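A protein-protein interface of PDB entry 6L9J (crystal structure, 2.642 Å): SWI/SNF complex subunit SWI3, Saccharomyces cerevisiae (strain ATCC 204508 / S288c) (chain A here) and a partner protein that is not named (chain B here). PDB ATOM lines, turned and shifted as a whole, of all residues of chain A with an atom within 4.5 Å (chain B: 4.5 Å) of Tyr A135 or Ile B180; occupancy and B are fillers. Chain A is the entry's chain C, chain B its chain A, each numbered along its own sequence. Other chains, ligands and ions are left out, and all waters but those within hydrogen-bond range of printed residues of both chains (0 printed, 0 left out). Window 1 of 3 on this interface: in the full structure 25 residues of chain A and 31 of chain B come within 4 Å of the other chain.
The side-chain hydroxyl of Thr B181 sits at hydrogen-bond distance from the side-chain carboxylate of Asp B184, 3.1 Å away.
OH of Tyr A135 lies within hydrogen-bond range of O of Ser A161 (2.7 Å).
Among the printed residues, merely in contact across the chains: Val A131 with Leu B182 (3.9 Å), Val A131 with Val B185 (3.9 Å), Arg A134 with Val B185 (3.2 Å), Tyr A135 with Ile B180 (3.6 Å), Tyr A135 with Val B185 (3.5 Å), Val A160 with Val B185 (3.1 Å), Ser A161 with Ile B180 (3.1 Å), Ser A161 with Asp B184 (3.6 Å) and Gly A162 with Ile B180 (3.3 Å).
The side-chain hydroxyl (OG) of Ser A126 sits close to the side-chain hydroxyl (OG1) of Thr B179, 3.5 Å away.
N of Ile B180 sits at hydrogen-bond distance from OG of Ser A126 (2.8 Å).
NH1 of Arg A134 sits at hydrogen-bond distance from O of Leu B182 (2.6 Å).
N of Ser A161 sits at hydrogen-bond distance from O of Val B185.
Hydrophobic or aromatic side chains of chain A that line the printed part of chain B: Val A131, Tyr A135 and Val A160.
Among the printed residues, no Asp or Glu carboxylate lies within 4 Å of a Lys or Arg side-chain nitrogen of the other chain.
Phe A119 touches none of the printed residues of chain B.
Of the printed residues of chain B, Arg A134 touches Leu B182 (2.6 Å) and Val B185 (3.2 Å).
Of chain B, only Ile B180 and Val B185 come within 4 Å of Tyr A135.
Printed residues of chain A within 4 Å of Thr B179: Ser A126.
Ile B180 touches four residues of chain A.
The nearest printed residue of chain B that does not touch Tyr A135 is Thr B181 (6.5 Å).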
ATOM      1  N   PHE A 119     -19.223  24.444  -7.535  1.00  0.00           N
ATOM      2  CA  PHE A 119     -20.045  23.813  -6.511  1.00  0.00           C
ATOM      3  C   PHE A 119     -21.004  22.762  -7.064  1.00  0.00           C
ATOM      4  O   PHE A 119     -21.730  22.133  -6.292  1.00  0.00           O
ATOM      5  CB  PHE A 119     -20.826  24.886  -5.748  1.00  0.00           C
ATOM      6  CG  PHE A 119     -19.947  25.909  -5.105  1.00  0.00           C
ATOM      7  CD1 PHE A 119     -19.359  25.664  -3.878  1.00  0.00           C
ATOM      8  CD2 PHE A 119     -19.669  27.102  -5.746  1.00  0.00           C
ATOM      9  CE1 PHE A 119     -18.528  26.589  -3.310  1.00  0.00           C
ATOM     10  CE2 PHE A 119     -18.836  28.031  -5.164  1.00  0.00           C
ATOM     11  CZ  PHE A 119     -18.268  27.769  -3.949  1.00  0.00           C
ATOM     12  N   PRO A 125     -16.471  16.906  -2.167  1.00  0.00           N
ATOM     13  CA  PRO A 125     -17.417  16.907  -1.043  1.00  0.00           C
ATOM     14  C   PRO A 125     -17.527  18.245  -0.319  1.00  0.00           C
ATOM     15  O   PRO A 125     -18.598  18.548   0.219  1.00  0.00           O
ATOM     16  CB  PRO A 125     -16.887  15.792  -0.126  1.00  0.00           C
ATOM     17  CG  PRO A 125     -15.626  15.310  -0.727  1.00  0.00           C
ATOM     18  CD  PRO A 125     -15.584  15.737  -2.146  1.00  0.00           C
ATOM     19  N   SER A 126     -16.480  19.071  -0.305  1.00  0.00           N
ATOM     20  CA  SER A 126     -16.553  20.353   0.389  1.00  0.00           C
ATOM     21  C   SER A 126     -17.295  21.431  -0.393  1.00  0.00           C
ATOM     22  O   SER A 126     -17.568  22.495   0.176  1.00  0.00           O
ATOM     23  CB  SER A 126     -15.151  20.880   0.725  1.00  0.00           C
ATOM     24  OG  SER A 126     -14.546  20.152   1.776  1.00  0.00           O
ATOM     25  N   VAL A 131     -23.698  23.864   0.775  1.00  0.00           N
ATOM     26  CA  VAL A 131     -22.750  24.858   1.252  1.00  0.00           C
ATOM     27  C   VAL A 131     -22.769  26.088   0.356  1.00  0.00           C
ATOM     28  O   VAL A 131     -22.618  27.212   0.834  1.00  0.00           O
ATOM     29  CB  VAL A 131     -21.337  24.270   1.380  1.00  0.00           C
ATOM     30  CG1 VAL A 131     -21.379  22.771   1.441  1.00  0.00           C
ATOM     31  CG2 VAL A 131     -20.487  24.737   0.262  1.00  0.00           C
ATOM     32  N   TYR A 132     -22.965  25.919  -0.945  1.00  0.00           N
ATOM     33  CA  TYR A 132     -23.107  27.093  -1.798  1.00  0.00           C
ATOM     34  C   TYR A 132     -24.160  28.053  -1.244  1.00  0.00           C
ATOM     35  O   TYR A 132     -23.949  29.268  -1.211  1.00  0.00           O
ATOM     36  CB  TYR A 132     -23.446  26.669  -3.244  1.00  0.00           C
ATOM     37  CG  TYR A 132     -23.811  27.842  -4.117  1.00  0.00           C
ATOM     38  CD1 TYR A 132     -22.844  28.632  -4.692  1.00  0.00           C
ATOM     39  CD2 TYR A 132     -25.124  28.180  -4.324  1.00  0.00           C
ATOM     40  CE1 TYR A 132     -23.180  29.715  -5.451  1.00  0.00           C
ATOM     41  CE2 TYR A 132     -25.464  29.258  -5.077  1.00  0.00           C
ATOM     42  CZ  TYR A 132     -24.494  30.023  -5.634  1.00  0.00           C
ATOM     43  OH  TYR A 132     -24.854  31.106  -6.387  1.00  0.00           O
ATOM     44  N   MET A 133     -25.310  27.532  -0.817  1.00  0.00           N
ATOM     45  CA  MET A 133     -26.403  28.410  -0.412  1.00  0.00           C
ATOM     46  C   MET A 133     -26.054  29.135   0.879  1.00  0.00           C
ATOM     47  O   MET A 133     -26.384  30.313   1.059  1.00  0.00           O
ATOM     48  CB  MET A 133     -27.695  27.601  -0.251  1.00  0.00           C
ATOM     49  CG  MET A 133     -28.858  28.031  -1.156  1.00  0.00           C
ATOM     50  SD  MET A 133     -30.468  27.358  -0.665  1.00  0.00           S
ATOM     51  CE  MET A 133     -30.019  25.637  -0.505  1.00  0.00           C
ATOM     52  N   ARG A 134     -25.372  28.448   1.785  1.00  0.00           N
ATOM     53  CA  ARG A 134     -24.880  29.112   2.979  1.00  0.00           C
ATOM     54  C   ARG A 134     -23.949  30.257   2.622  1.00  0.00           C
ATOM     55  O   ARG A 134     -24.246  31.417   2.920  1.00  0.00           O
ATOM     56  CB  ARG A 134     -24.195  28.107   3.888  1.00  0.00           C
ATOM     57  CG  ARG A 134     -24.061  28.612   5.314  1.00  0.00           C
ATOM     58  CD  ARG A 134     -24.173  27.466   6.283  1.00  0.00           C
ATOM     59  NE  ARG A 134     -25.546  27.249   6.706  1.00  0.00           N
ATOM     60  CZ  ARG A 134     -25.958  26.160   7.338  1.00  0.00           C
ATOM     61  NH1 ARG A 134     -25.103  25.187   7.601  1.00  0.00           N
ATOM     62  NH2 ARG A 134     -27.222  26.040   7.698  1.00  0.00           N
ATOM     63  N   TYR A 135     -22.814  29.954   1.974  1.00  0.00           N
ATOM     64  CA  TYR A 135     -21.886  31.018   1.593  1.00  0.00           C
ATOM     65  C   TYR A 135     -22.629  32.161   0.929  1.00  0.00           C
ATOM     66  O   TYR A 135     -22.296  33.334   1.124  1.00  0.00           O
ATOM     67  CB  TYR A 135     -20.809  30.532   0.623  1.00  0.00           C
ATOM     68  CG  TYR A 135     -19.864  29.454   1.078  1.00  0.00           C
ATOM     69  CD1 TYR A 135     -19.837  29.019   2.368  1.00  0.00           C
ATOM     70  CD2 TYR A 135     -18.989  28.869   0.181  1.00  0.00           C
ATOM     71  CE1 TYR A 135     -18.968  28.024   2.750  1.00  0.00           C
ATOM     72  CE2 TYR A 135     -18.127  27.887   0.556  1.00  0.00           C
ATOM     73  CZ  TYR A 135     -18.117  27.465   1.839  1.00  0.00           C
ATOM     74  OH  TYR A 135     -17.250  26.474   2.215  1.00  0.00           O
ATOM     75  N   ARG A 136     -23.647  31.838   0.136  1.00  0.00           N
ATOM     76  CA  ARG A 136     -24.258  32.828  -0.737  1.00  0.00           C
ATOM     77  C   ARG A 136     -25.306  33.632  -0.001  1.00  0.00           C
ATOM     78  O   ARG A 136     -25.420  34.840  -0.211  1.00  0.00           O
ATOM     79  CB  ARG A 136     -24.860  32.146  -1.969  1.00  0.00           C
ATOM     80  CG  ARG A 136     -25.430  33.120  -2.964  1.00  0.00           C
ATOM     81  CD  ARG A 136     -26.924  33.047  -2.971  1.00  0.00           C
ATOM     82  NE  ARG A 136     -27.375  31.663  -3.009  1.00  0.00           N
ATOM     83  CZ  ARG A 136     -28.602  31.290  -3.342  1.00  0.00           C
ATOM     84  NH1 ARG A 136     -29.499  32.193  -3.665  1.00  0.00           N
ATOM     85  NH2 ARG A 136     -28.932  30.015  -3.350  1.00  0.00           N
ATOM     86  N   ASN A 137     -26.075  32.980   0.865  1.00  0.00           N
ATOM     87  CA  ASN A 137     -27.074  33.714   1.627  1.00  0.00           C
ATOM     88  C   ASN A 137     -26.421  34.561   2.710  1.00  0.00           C
ATOM     89  O   ASN A 137     -26.824  35.706   2.927  1.00  0.00           O
ATOM     90  CB  ASN A 137     -28.105  32.745   2.196  1.00  0.00           C
ATOM     91  CG  ASN A 137     -29.033  32.209   1.118  1.00  0.00           C
ATOM     92  OD1 ASN A 137     -28.867  32.532  -0.054  1.00  0.00           O
ATOM     93  ND2 ASN A 137     -30.000  31.392   1.503  1.00  0.00           N
ATOM     94  N   PHE A 138     -25.375  34.046   3.360  1.00  0.00           N
ATOM     95  CA  PHE A 138     -24.661  34.865   4.329  1.00  0.00           C
ATOM     96  C   PHE A 138     -24.146  36.156   3.707  1.00  0.00           C
ATOM     97  O   PHE A 138     -24.250  37.225   4.322  1.00  0.00           O
ATOM     98  CB  PHE A 138     -23.499  34.104   4.951  1.00  0.00           C
ATOM     99  CG  PHE A 138     -22.720  34.927   5.926  1.00  0.00           C
ATOM    100  CD1 PHE A 138     -21.640  35.673   5.512  1.00  0.00           C
ATOM    101  CD2 PHE A 138     -23.097  34.994   7.254  1.00  0.00           C
ATOM    102  CE1 PHE A 138     -20.939  36.447   6.408  1.00  0.00           C
ATOM    103  CE2 PHE A 138     -22.397  35.766   8.141  1.00  0.00           C
ATOM    104  CZ  PHE A 138     -21.323  36.489   7.716  1.00  0.00           C
ATOM    105  N   MET A 139     -23.559  36.080   2.504  1.00  0.00           N
ATOM    106  CA  MET A 139     -23.057  37.298   1.874  1.00  0.00           C
ATOM    107  C   MET A 139     -24.207  38.234   1.526  1.00  0.00           C
ATOM    108  O   MET A 139     -24.100  39.452   1.708  1.00  0.00           O
ATOM    109  CB  MET A 139     -22.220  36.974   0.626  1.00  0.00           C
ATOM    110  CG  MET A 139     -21.071  35.966   0.801  1.00  0.00           C
ATOM    111  SD  MET A 139     -19.835  35.985  -0.525  1.00  0.00           S
ATOM    112  CE  MET A 139     -20.221  37.548  -1.238  1.00  0.00           C
ATOM    113  N   VAL A 160     -17.150  32.442   7.361  1.00  0.00           N
ATOM    114  CA  VAL A 160     -17.410  31.118   6.801  1.00  0.00           C
ATOM    115  C   VAL A 160     -16.108  30.441   6.391  1.00  0.00           C
ATOM    116  O   VAL A 160     -15.228  31.064   5.794  1.00  0.00           O
ATOM    117  CB  VAL A 160     -18.388  31.180   5.607  1.00  0.00           C
ATOM    118  CG1 VAL A 160     -19.647  31.923   5.996  1.00  0.00           C
ATOM    119  CG2 VAL A 160     -17.728  31.806   4.399  1.00  0.00           C
ATOM    120  N   SER A 161     -16.008  29.152   6.698  1.00  0.00           N
ATOM    121  CA  SER A 161     -14.898  28.311   6.278  1.00  0.00           C
ATOM    122  C   SER A 161     -15.074  27.852   4.829  1.00  0.00           C
ATOM    123  O   SER A 161     -16.190  27.590   4.379  1.00  0.00           O
ATOM    124  CB  SER A 161     -14.810  27.105   7.208  1.00  0.00           C
ATOM    125  OG  SER A 161     -13.899  26.137   6.737  1.00  0.00           O
ATOM    126  N   GLY A 162     -13.968  27.750   4.106  1.00  0.00           N
ATOM    127  CA  GLY A 162     -13.948  27.418   2.691  1.00  0.00           C
ATOM    128  C   GLY A 162     -12.868  28.190   1.952  1.00  0.00           C
ATOM    129  O   GLY A 162     -12.375  29.215   2.410  1.00  0.00           O
ATOM    130  N   LEU A 167     -14.509  31.933  -2.449  1.00  0.00           N
ATOM    131  CA  LEU A 167     -15.353  32.998  -1.904  1.00  0.00           C
ATOM    132  C   LEU A 167     -15.115  34.333  -2.584  1.00  0.00           C
ATOM    133  O   LEU A 167     -16.044  35.130  -2.704  1.00  0.00           O
ATOM    134  CB  LEU A 167     -15.125  33.166  -0.404  1.00  0.00           C
ATOM    135  CG  LEU A 167     -15.439  32.033   0.565  1.00  0.00           C
ATOM    136  CD1 LEU A 167     -14.926  32.418   1.922  1.00  0.00           C
ATOM    137  CD2 LEU A 167     -16.927  31.794   0.593  1.00  0.00           C
ATOM    138  N   LEU A 170     -17.393  33.840  -5.614  1.00  0.00           N
ATOM    139  CA  LEU A 170     -18.809  33.980  -5.283  1.00  0.00           C
ATOM    140  C   LEU A 170     -19.163  35.437  -5.044  1.00  0.00           C
ATOM    141  O   LEU A 170     -20.201  35.918  -5.509  1.00  0.00           O
ATOM    142  CB  LEU A 170     -19.154  33.121  -4.068  1.00  0.00           C
ATOM    143  CG  LEU A 170     -20.556  33.111  -3.456  1.00  0.00           C
ATOM    144  CD1 LEU A 170     -21.643  33.389  -4.466  1.00  0.00           C
ATOM    145  CD2 LEU A 170     -20.797  31.779  -2.788  1.00  0.00           C
ATOM    146  N   ARG B  90      -7.051  22.288   0.560  1.00  0.00           N
ATOM    147  CA  ARG B  90      -6.891  23.639   1.065  1.00  0.00           C
ATOM    148  C   ARG B  90      -5.737  23.716   2.054  1.00  0.00           C
ATOM    149  O   ARG B  90      -5.547  22.827   2.880  1.00  0.00           O
ATOM    150  CB  ARG B  90      -8.183  24.109   1.722  1.00  0.00           C
ATOM    151  CG  ARG B  90      -9.246  24.543   0.742  1.00  0.00           C
ATOM    152  CD  ARG B  90     -10.567  24.744   1.453  1.00  0.00           C
ATOM    153  NE  ARG B  90     -11.027  23.495   2.037  1.00  0.00           N
ATOM    154  CZ  ARG B  90     -11.077  23.251   3.335  1.00  0.00           C
ATOM    155  NH1 ARG B  90     -10.713  24.179   4.202  1.00  0.00           N
ATOM    156  NH2 ARG B  90     -11.508  22.081   3.765  1.00  0.00           N
ATOM    157  N   PRO B 178      -9.582  20.301   7.037  1.00  0.00           N
ATOM    158  CA  PRO B 178     -10.526  19.184   6.953  1.00  0.00           C
ATOM    159  C   PRO B 178     -11.684  19.514   6.024  1.00  0.00           C
ATOM    160  O   PRO B 178     -11.882  20.655   5.622  1.00  0.00           O
ATOM    161  CB  PRO B 178     -10.995  19.028   8.399  1.00  0.00           C
ATOM    162  CG  PRO B 178     -10.888  20.395   8.951  1.00  0.00           C
ATOM    163  CD  PRO B 178      -9.690  21.018   8.321  1.00  0.00           C
ATOM    164  N   THR B 179     -12.462  18.482   5.701  1.00  0.00           N
ATOM    165  CA  THR B 179     -13.540  18.617   4.729  1.00  0.00           C
ATOM    166  C   THR B 179     -14.711  19.387   5.314  1.00  0.00           C
ATOM    167  O   THR B 179     -15.047  19.244   6.483  1.00  0.00           O
ATOM    168  CB  THR B 179     -14.011  17.243   4.249  1.00  0.00           C
ATOM    169  OG1 THR B 179     -13.526  17.017   2.921  1.00  0.00           O
ATOM    170  CG2 THR B 179     -15.522  17.164   4.231  1.00  0.00           C
ATOM    171  N   ILE B 180     -15.364  20.173   4.468  1.00  0.00           N
ATOM    172  CA  ILE B 180     -16.348  21.158   4.900  1.00  0.00           C
ATOM    173  C   ILE B 180     -17.738  20.559   4.718  1.00  0.00           C
ATOM    174  O   ILE B 180     -18.377  20.747   3.688  1.00  0.00           O
ATOM    175  CB  ILE B 180     -16.198  22.464   4.132  1.00  0.00           C
ATOM    176  CG1 ILE B 180     -14.940  23.192   4.580  1.00  0.00           C
ATOM    177  CG2 ILE B 180     -17.404  23.335   4.309  1.00  0.00           C
ATOM    178  CD1 ILE B 180     -14.928  24.640   4.209  1.00  0.00           C
ATOM    179  N   THR B 181     -18.238  19.856   5.733  1.00  0.00           N
ATOM    180  CA  THR B 181     -19.652  19.507   5.712  1.00  0.00           C
ATOM    181  C   THR B 181     -20.469  20.782   5.889  1.00  0.00           C
ATOM    182  O   THR B 181     -19.927  21.888   5.932  1.00  0.00           O
ATOM    183  CB  THR B 181     -19.996  18.481   6.789  1.00  0.00           C
ATOM    184  OG1 THR B 181     -19.863  19.080   8.075  1.00  0.00           O
ATOM    185  CG2 THR B 181     -19.089  17.272   6.705  1.00  0.00           C
ATOM    186  N   LEU B 182     -21.793  20.648   5.971  1.00  0.00           N
ATOM    187  CA  LEU B 182     -22.616  21.845   6.086  1.00  0.00           C
ATOM    188  C   LEU B 182     -22.679  22.365   7.511  1.00  0.00           C
ATOM    189  O   LEU B 182     -23.072  23.515   7.718  1.00  0.00           O
ATOM    190  CB  LEU B 182     -24.038  21.603   5.578  1.00  0.00           C
ATOM    191  CG  LEU B 182     -24.941  22.845   5.691  1.00  0.00           C
ATOM    192  CD1 LEU B 182     -24.723  23.787   4.537  1.00  0.00           C
ATOM    193  CD2 LEU B 182     -26.412  22.504   5.812  1.00  0.00           C
ATOM    194  N   ASP B 184     -20.003  22.793   9.183  1.00  0.00           N
ATOM    195  CA  ASP B 184     -18.713  23.457   9.304  1.00  0.00           C
ATOM    196  C   ASP B 184     -18.663  24.797   8.593  1.00  0.00           C
ATOM    197  O   ASP B 184     -17.697  25.537   8.771  1.00  0.00           O
ATOM    198  CB  ASP B 184     -17.603  22.565   8.750  1.00  0.00           C
ATOM    199  CG  ASP B 184     -17.393  21.309   9.564  1.00  0.00           C
ATOM    200  OD1 ASP B 184     -17.162  20.243   8.974  1.00  0.00           O
ATOM    201  OD2 ASP B 184     -17.432  21.384  10.804  1.00  0.00           O
ATOM    202  N   VAL B 185     -19.668  25.124   7.790  1.00  0.00           N
ATOM    203  CA  VAL B 185     -19.617  26.353   7.008  1.00  0.00           C
ATOM    204  C   VAL B 185     -19.435  27.545   7.933  1.00  0.00           C
ATOM    205  O   VAL B 185     -18.501  28.334   7.781  1.00  0.00           O
ATOM    206  CB  VAL B 185     -20.877  26.492   6.133  1.00  0.00           C
ATOM    207  CG1 VAL B 185     -20.991  27.895   5.552  1.00  0.00           C
ATOM    208  CG2 VAL B 185     -20.856  25.475   5.024  1.00  0.00           C
